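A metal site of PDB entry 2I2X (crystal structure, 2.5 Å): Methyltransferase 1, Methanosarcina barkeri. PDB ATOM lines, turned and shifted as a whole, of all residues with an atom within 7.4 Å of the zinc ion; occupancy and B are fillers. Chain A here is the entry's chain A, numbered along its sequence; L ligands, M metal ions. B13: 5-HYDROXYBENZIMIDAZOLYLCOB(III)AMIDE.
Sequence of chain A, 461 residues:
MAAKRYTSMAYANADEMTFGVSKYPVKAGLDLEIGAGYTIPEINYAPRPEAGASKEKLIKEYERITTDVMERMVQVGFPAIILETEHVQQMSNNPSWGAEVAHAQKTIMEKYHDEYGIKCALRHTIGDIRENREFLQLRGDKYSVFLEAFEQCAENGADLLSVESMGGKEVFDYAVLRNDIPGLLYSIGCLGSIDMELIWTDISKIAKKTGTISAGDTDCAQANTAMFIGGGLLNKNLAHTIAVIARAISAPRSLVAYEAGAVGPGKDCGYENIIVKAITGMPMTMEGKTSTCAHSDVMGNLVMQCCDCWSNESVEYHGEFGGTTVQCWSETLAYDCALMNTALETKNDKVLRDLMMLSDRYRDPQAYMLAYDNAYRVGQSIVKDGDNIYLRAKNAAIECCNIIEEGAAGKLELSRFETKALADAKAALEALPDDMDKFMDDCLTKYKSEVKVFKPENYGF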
ATOM      1  N   GLU A  86     -15.477  15.732  31.922  1.00  0.00           N
ATOM      2  CA  GLU A  86     -15.732  15.311  30.549  1.00  0.00           C
ATOM      3  C   GLU A  86     -16.838  14.313  30.541  1.00  0.00           C
ATOM      4  O   GLU A  86     -16.624  13.184  30.931  1.00  0.00           O
ATOM      5  CB  GLU A  86     -14.498  14.657  29.935  1.00  0.00           C
ATOM      6  CG  GLU A  86     -13.360  15.640  29.789  1.00  0.00           C
ATOM      7  CD  GLU A  86     -12.151  15.071  29.114  1.00  0.00           C
ATOM      8  OE1 GLU A  86     -11.585  14.070  29.616  1.00  0.00           O
ATOM      9  OE2 GLU A  86     -11.744  15.632  28.077  1.00  0.00           O
ATOM     10  N   GLU A 164     -15.147  18.339  22.616  1.00  0.00           N
ATOM     11  CA  GLU A 164     -14.135  17.903  21.669  1.00  0.00           C
ATOM     12  C   GLU A 164     -14.870  17.455  20.399  1.00  0.00           C
ATOM     13  O   GLU A 164     -15.297  16.314  20.316  1.00  0.00           O
ATOM     14  CB  GLU A 164     -13.365  16.719  22.227  1.00  0.00           C
ATOM     15  CG  GLU A 164     -13.195  16.797  23.699  1.00  0.00           C
ATOM     16  CD  GLU A 164     -11.855  16.256  24.156  1.00  0.00           C
ATOM     17  OE1 GLU A 164     -11.111  15.699  23.348  1.00  0.00           O
ATOM     18  OE2 GLU A 164     -11.548  16.366  25.358  1.00  0.00           O
ATOM     19  N   THR A 218     -11.083  21.681  20.773  1.00  0.00           N
ATOM     20  CA  THR A 218      -9.747  21.058  20.657  1.00  0.00           C
ATOM     21  C   THR A 218      -9.806  20.181  19.477  1.00  0.00           C
ATOM     22  O   THR A 218     -10.756  19.387  19.332  1.00  0.00           O
ATOM     23  CB  THR A 218      -9.540  19.877  21.644  1.00  0.00           C
ATOM     24  OG1 THR A 218      -9.884  20.255  22.944  1.00  0.00           O
ATOM     25  CG2 THR A 218      -8.159  19.397  21.645  1.00  0.00           C
ATOM     26  N   ASP A 219      -8.725  20.195  18.715  1.00  0.00           N
ATOM     27  CA  ASP A 219      -8.631  19.228  17.658  1.00  0.00           C
ATOM     28  C   ASP A 219      -8.254  17.810  18.057  1.00  0.00           C
ATOM     29  O   ASP A 219      -7.601  17.098  17.265  1.00  0.00           O
ATOM     30  CB  ASP A 219      -7.707  19.678  16.567  1.00  0.00           C
ATOM     31  CG  ASP A 219      -8.094  19.093  15.244  1.00  0.00           C
ATOM     32  OD1 ASP A 219      -9.321  19.042  14.964  1.00  0.00           O
ATOM     33  OD2 ASP A 219      -7.178  18.679  14.497  1.00  0.00           O
ATOM     34  N   CYS A 220      -8.664  17.388  19.249  1.00  0.00           N
ATOM     35  CA  CYS A 220      -8.329  16.061  19.786  1.00  0.00           C
ATOM     36  C   CYS A 220      -8.597  14.923  18.818  1.00  0.00           C
ATOM     37  O   CYS A 220      -7.783  14.033  18.637  1.00  0.00           O
ATOM     38  CB  CYS A 220      -9.116  15.782  21.043  1.00  0.00           C
ATOM     39  SG  CYS A 220      -8.224  14.593  22.137  1.00  0.00           S
ATOM     40  N   ALA A 221      -9.769  14.987  18.173  1.00  0.00           N
ATOM     41  CA  ALA A 221     -10.248  13.926  17.305  1.00  0.00           C
ATOM     42  C   ALA A 221      -9.384  13.758  16.060  1.00  0.00           C
ATOM     43  O   ALA A 221      -9.494  12.735  15.378  1.00  0.00           O
ATOM     44  CB  ALA A 221     -11.725  14.133  16.956  1.00  0.00           C
ATOM     45  N   ASN A 224      -4.660  15.123  17.916  1.00  0.00           N
ATOM     46  CA  ASN A 224      -4.135  14.219  18.956  1.00  0.00           C
ATOM     47  C   ASN A 224      -4.054  12.769  18.475  1.00  0.00           C
ATOM     48  O   ASN A 224      -3.101  12.062  18.826  1.00  0.00           O
ATOM     49  CB  ASN A 224      -4.783  14.355  20.376  1.00  0.00           C
ATOM     50  CG  ASN A 224      -4.495  15.750  21.038  1.00  0.00           C
ATOM     51  OD1 ASN A 224      -3.482  16.437  20.733  1.00  0.00           O
ATOM     52  ND2 ASN A 224      -5.410  16.159  21.956  1.00  0.00           N
ATOM     53  N   LYS A 267      -9.647  24.083  25.684  1.00  0.00           N
ATOM     54  CA  LYS A 267      -9.389  22.757  26.217  1.00  0.00           C
ATOM     55  C   LYS A 267      -7.954  22.339  26.275  1.00  0.00           C
ATOM     56  O   LYS A 267      -7.200  22.548  25.341  1.00  0.00           O
ATOM     57  CB  LYS A 267     -10.133  21.709  25.393  1.00  0.00           C
ATOM     58  CG  LYS A 267     -11.586  21.570  25.781  1.00  0.00           C
ATOM     59  CD  LYS A 267     -11.707  20.600  26.923  1.00  0.00           C
ATOM     60  CE  LYS A 267     -11.442  19.200  26.439  1.00  0.00           C
ATOM     61  NZ  LYS A 267     -11.235  18.323  27.608  1.00  0.00           N
ATOM     62  N   ASP A 268      -7.628  21.679  27.376  1.00  0.00           N
ATOM     63  CA  ASP A 268      -6.305  21.166  27.704  1.00  0.00           C
ATOM     64  C   ASP A 268      -5.614  20.382  26.606  1.00  0.00           C
ATOM     65  O   ASP A 268      -4.420  20.582  26.343  1.00  0.00           O
ATOM     66  CB  ASP A 268      -6.392  20.336  28.999  1.00  0.00           C
ATOM     67  CG  ASP A 268      -7.417  19.225  28.910  1.00  0.00           C
ATOM     68  OD1 ASP A 268      -8.091  19.090  27.857  1.00  0.00           O
ATOM     69  OD2 ASP A 268      -7.553  18.470  29.891  1.00  0.00           O
ATOM     70  N   CYS A 269      -6.330  19.478  25.969  1.00  0.00           N
ATOM     71  CA  CYS A 269      -5.711  18.624  24.949  1.00  0.00           C
ATOM     72  C   CYS A 269      -5.495  19.349  23.611  1.00  0.00           C
ATOM     73  O   CYS A 269      -4.976  18.759  22.641  1.00  0.00           O
ATOM     74  CB  CYS A 269      -6.498  17.325  24.752  1.00  0.00           C
ATOM     75  SG  CYS A 269      -8.230  17.556  24.294  1.00  0.00           S
ATOM     76  N   GLY A 270      -5.856  20.621  23.579  1.00  0.00           N
ATOM     77  CA  GLY A 270      -5.565  21.508  22.448  1.00  0.00           C
ATOM     78  C   GLY A 270      -4.116  21.977  22.496  1.00  0.00           C
ATOM     79  O   GLY A 270      -3.834  23.135  22.817  1.00  0.00           O
ATOM     80  N   GLU A 287      -1.610  20.746  28.735  1.00  0.00           N
ATOM     81  CA  GLU A 287      -1.289  19.518  29.457  1.00  0.00           C
ATOM     82  C   GLU A 287       0.011  18.957  28.913  1.00  0.00           C
ATOM     83  O   GLU A 287       0.257  18.997  27.701  1.00  0.00           O
ATOM     84  CB  GLU A 287      -2.378  18.466  29.262  1.00  0.00           C
ATOM     85  CG  GLU A 287      -2.540  17.996  27.825  1.00  0.00           C
ATOM     86  CD  GLU A 287      -3.819  17.214  27.617  1.00  0.00           C
ATOM     87  OE1 GLU A 287      -4.857  17.636  28.150  1.00  0.00           O
ATOM     88  OE2 GLU A 287      -3.781  16.159  26.941  1.00  0.00           O
ATOM     89  N   HIS A 295      -1.511   9.895  29.051  1.00  0.00           N
ATOM     90  CA  HIS A 295      -0.701   9.538  27.868  1.00  0.00           C
ATOM     91  C   HIS A 295       0.653  10.160  27.913  1.00  0.00           C
ATOM     92  O   HIS A 295       0.860  11.156  28.565  1.00  0.00           O
ATOM     93  CB  HIS A 295      -1.383   9.985  26.522  1.00  0.00           C
ATOM     94  CG  HIS A 295      -1.727  11.444  26.464  1.00  0.00           C
ATOM     95  ND1 HIS A 295      -0.805  12.424  26.135  1.00  0.00           N
ATOM     96  CD2 HIS A 295      -2.875  12.100  26.744  1.00  0.00           C
ATOM     97  CE1 HIS A 295      -1.379  13.608  26.207  1.00  0.00           C
ATOM     98  NE2 HIS A 295      -2.636  13.440  26.564  1.00  0.00           N
ATOM     99  N   GLU A 313      -5.228  15.920  32.050  1.00  0.00           N
ATOM    100  CA  GLU A 313      -5.930  15.339  30.895  1.00  0.00           C
ATOM    101  C   GLU A 313      -7.027  14.402  31.336  1.00  0.00           C
ATOM    102  O   GLU A 313      -8.205  14.640  31.091  1.00  0.00           O
ATOM    103  CB  GLU A 313      -4.956  14.666  29.919  1.00  0.00           C
ATOM    104  CG  GLU A 313      -5.603  13.886  28.773  1.00  0.00           C
ATOM    105  CD  GLU A 313      -6.543  14.725  27.892  1.00  0.00           C
ATOM    106  OE1 GLU A 313      -7.305  14.091  27.115  1.00  0.00           O
ATOM    107  OE2 GLU A 313      -6.541  15.987  27.965  1.00  0.00           O
HETATM  108  O5  B13 L   1      -4.654  -0.470  21.287  1.00  0.00           O
HETATM  109  P   B13 L   1      -4.777   0.004  19.897  1.00  0.00           P
HETATM  110  O4  B13 L   1      -6.076   0.435  19.405  1.00  0.00           O
HETATM  111  O2  B13 L   1      -4.041  -1.041  18.897  1.00  0.00           O
HETATM  112  C3R B13 L   1      -2.829  -1.744  19.221  1.00  0.00           C
HETATM  113  C4R B13 L   1      -2.359  -2.275  17.827  1.00  0.00           C
HETATM  114  C5R B13 L   1      -1.380  -1.982  17.173  1.00  0.00           C
HETATM  115  O8R B13 L   1      -0.044  -2.687  17.602  1.00  0.00           O
HETATM  116  O6R B13 L   1      -3.248  -3.336  17.579  1.00  0.00           O
HETATM  117  C1R B13 L   1      -3.290  -4.031  18.839  1.00  0.00           C
HETATM  118  N1B B13 L   1      -4.528  -4.889  19.065  1.00  0.00           N
HETATM  119  C2B B13 L   1      -5.735  -4.169  18.916  1.00  0.00           C
HETATM  120  N3B B13 L   1      -6.743  -5.003  18.676  1.00  0.00           N
HETATM  121  C9B B13 L   1      -6.207  -6.281  18.623  1.00  0.00           C
HETATM  122  C4B B13 L   1      -6.802  -7.548  18.384  1.00  0.00           C
HETATM  123  C5B B13 L   1      -5.949  -8.678  18.394  1.00  0.00           C
HETATM  124  O5B B13 L   1      -6.532 -10.047  18.155  1.00  0.00           O
HETATM  125  C6B B13 L   1      -4.527  -8.538  18.641  1.00  0.00           C
HETATM  126  C7B B13 L   1      -3.941  -7.313  18.865  1.00  0.00           C
HETATM  127  C8B B13 L   1      -4.811  -6.197  18.837  1.00  0.00           C
HETATM  128  C2R B13 L   1      -2.970  -3.013  19.972  1.00  0.00           C
HETATM  129  O7R B13 L   1      -3.653  -3.159  21.160  1.00  0.00           O
HETATM  130  O3  B13 L   1      -3.886   1.315  19.703  1.00  0.00           O
HETATM  131  C2P B13 L   1      -3.729   2.036  18.515  1.00  0.00           C
HETATM  132  C3P B13 L   1      -2.564   1.466  17.748  1.00  0.00           C
HETATM  133  C1P B13 L   1      -3.388   3.455  18.904  1.00  0.00           C
HETATM  134  N59 B13 L   1      -4.204   3.953  20.018  1.00  0.00           N
HETATM  135  C57 B13 L   1      -5.311   4.594  19.754  1.00  0.00           C
HETATM  136  O58 B13 L   1      -5.695   4.793  18.591  1.00  0.00           O
HETATM  137  C56 B13 L   1      -6.074   5.098  20.946  1.00  0.00           C
HETATM  138  C55 B13 L   1      -5.572   6.498  21.296  1.00  0.00           C
HETATM  139  C17 B13 L   1      -6.574   7.484  22.057  1.00  0.00           C
HETATM  140  C54 B13 L   1      -5.925   8.893  22.000  1.00  0.00           C
HETATM  141  C18 B13 L   1      -6.828   7.001  23.527  1.00  0.00           C
HETATM  142  C60 B13 L   1      -5.717   7.230  24.591  1.00  0.00           C
HETATM  143  C61 B13 L   1      -5.187   6.137  25.413  1.00  0.00           C
HETATM  144  N62 B13 L   1      -5.258   4.944  24.881  1.00  0.00           N
HETATM  145  O63 B13 L   1      -4.710   6.351  26.562  1.00  0.00           O
HETATM  146  C19 B13 L   1      -8.228   7.557  23.869  1.00  0.00           C
HETATM  147  C1  B13 L   1      -9.145   6.815  24.831  1.00  0.00           C
HETATM  148  C2  B13 L   1      -8.993   7.026  26.408  1.00  0.00           C
HETATM  149  C3  B13 L   1     -10.491   7.082  26.869  1.00  0.00           C
HETATM  150  C4  B13 L   1     -11.186   7.612  25.629  1.00  0.00           C
HETATM  151  C5  B13 L   1     -12.489   8.245  25.638  1.00  0.00           C
HETATM  152  C35 B13 L   1     -13.095   8.589  27.027  1.00  0.00           C
HETATM  153  C30 B13 L   1     -11.112   5.764  27.482  1.00  0.00           C
HETATM  154  C31 B13 L   1     -11.259   5.887  28.979  1.00  0.00           C
HETATM  155  C32 B13 L   1     -11.553   4.603  29.642  1.00  0.00           C
HETATM  156  N33 B13 L   1     -10.802   3.518  29.513  1.00  0.00           N
HETATM  157  O34 B13 L   1     -12.578   4.729  30.333  1.00  0.00           O
HETATM  158  C26 B13 L   1      -8.385   8.463  26.662  1.00  0.00           C
HETATM  159  C27 B13 L   1      -8.064   8.846  28.090  1.00  0.00           C
HETATM  160  N29 B13 L   1      -6.827   9.198  28.388  1.00  0.00           N
HETATM  161  O28 B13 L   1      -8.974   8.837  28.965  1.00  0.00           O
HETATM  162  C25 B13 L   1      -8.085   5.928  27.115  1.00  0.00           C
HETATM  163  C20 B13 L   1      -9.314   5.283  24.339  1.00  0.00           C
HETATM  164  N21 B13 L   1     -10.462   7.454  24.534  1.00  0.00           N
HETATM  165  N24 B13 L   1      -8.942   7.601  22.571  1.00  0.00           N
HETATM  166 CO   B13 L   1     -10.741   7.879  22.771  1.00  0.00          CO
HETATM  167  C16 B13 L   1      -8.079   7.668  21.574  1.00  0.00           C
HETATM  168  C15 B13 L   1      -8.478   7.915  20.231  1.00  0.00           C
HETATM  169  C53 B13 L   1      -7.451   7.922  19.121  1.00  0.00           C
HETATM  170  C14 B13 L   1      -9.828   8.187  19.956  1.00  0.00           C
HETATM  171  N23 B13 L   1     -10.843   8.283  20.897  1.00  0.00           N
HETATM  172  C13 B13 L   1     -10.432   8.453  18.561  1.00  0.00           C
HETATM  173  C48 B13 L   1     -10.585   7.100  17.804  1.00  0.00           C
HETATM  174  C49 B13 L   1      -9.818   6.965  16.471  1.00  0.00           C
HETATM  175  C50 B13 L   1     -10.233   5.683  15.767  1.00  0.00           C
HETATM  176  N52 B13 L   1     -10.990   5.800  14.712  1.00  0.00           N
HETATM  177  O51 B13 L   1      -9.840   4.573  16.160  1.00  0.00           O
HETATM  178  C12 B13 L   1     -11.775   9.146  18.811  1.00  0.00           C
HETATM  179  C46 B13 L   1     -11.541  10.704  18.703  1.00  0.00           C
HETATM  180  C47 B13 L   1     -12.992   8.881  17.843  1.00  0.00           C
HETATM  181  C11 B13 L   1     -11.976   8.759  20.290  1.00  0.00           C
HETATM  182  C10 B13 L   1     -13.162   8.925  20.938  1.00  0.00           C
HETATM  183  C9  B13 L   1     -13.394   8.704  22.264  1.00  0.00           C
HETATM  184  N22 B13 L   1     -12.490   8.395  23.188  1.00  0.00           N
HETATM  185  C8  B13 L   1     -14.805   8.826  22.792  1.00  0.00           C
HETATM  186  C41 B13 L   1     -15.510   7.424  22.719  1.00  0.00           C
HETATM  187  C42 B13 L   1     -16.379   7.039  21.541  1.00  0.00           C
HETATM  188  C43 B13 L   1     -16.608   5.523  21.601  1.00  0.00           C
HETATM  189  N45 B13 L   1     -17.860   5.173  21.675  1.00  0.00           N
HETATM  190  O44 B13 L   1     -15.667   4.701  21.569  1.00  0.00           O
HETATM  191  C7  B13 L   1     -14.530   9.170  24.284  1.00  0.00           C
HETATM  192  C6  B13 L   1     -13.089   8.553  24.465  1.00  0.00           C
HETATM  193  C36 B13 L   1     -15.782   8.954  25.233  1.00  0.00           C
HETATM  194  C37 B13 L   1     -14.240  10.733  24.264  1.00  0.00           C
HETATM  195  C38 B13 L   1     -15.351  11.724  24.409  1.00  0.00           C
HETATM  196  O39 B13 L   1     -15.283  12.525  25.356  1.00  0.00           O
HETATM  197  N40 B13 L   1     -16.361  11.750  23.590  1.00  0.00           N
HETATM  198 ZN    ZN M   1      -9.123  15.353  24.017  1.00  0.00          ZN
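Glu 313 touches the zinc ion.
Four residues have an atom within 4 Å of the zinc ion: Glu 164, Cys 220, Cys 269 and Glu 313.
The side-chain amino group (NZ) of Lys 267 is in salt-bridge range of the side-chain carboxylate (OE2) of Glu 164, 3.0 Å away.
The side-chain sulfur (SG) of Cys 220 sits close to the side-chain amide nitrogen (ND2) of Asn 224, 3.2 Å away.
O of Cys 269 is in hydrogen-bond range of ND2 of Asn 224 (2.7 Å).
The side-chain hydroxyl (OG1) of Thr 218 lies close to the side-chain sulfur (SG) of Cys 269, 3.4 Å away.
OE1 of Glu 287 sits at hydrogen-bond distance from N of Cys 269 (3.2 Å).
The zinc ion is bound by the side-chain carboxylate (OE1) of Glu 164, the side-chain sulfur (SG) of Cys 220 and the side-chain sulfur (SG) of Cys 269.
The zinc ion has three donor atoms within binding distance.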
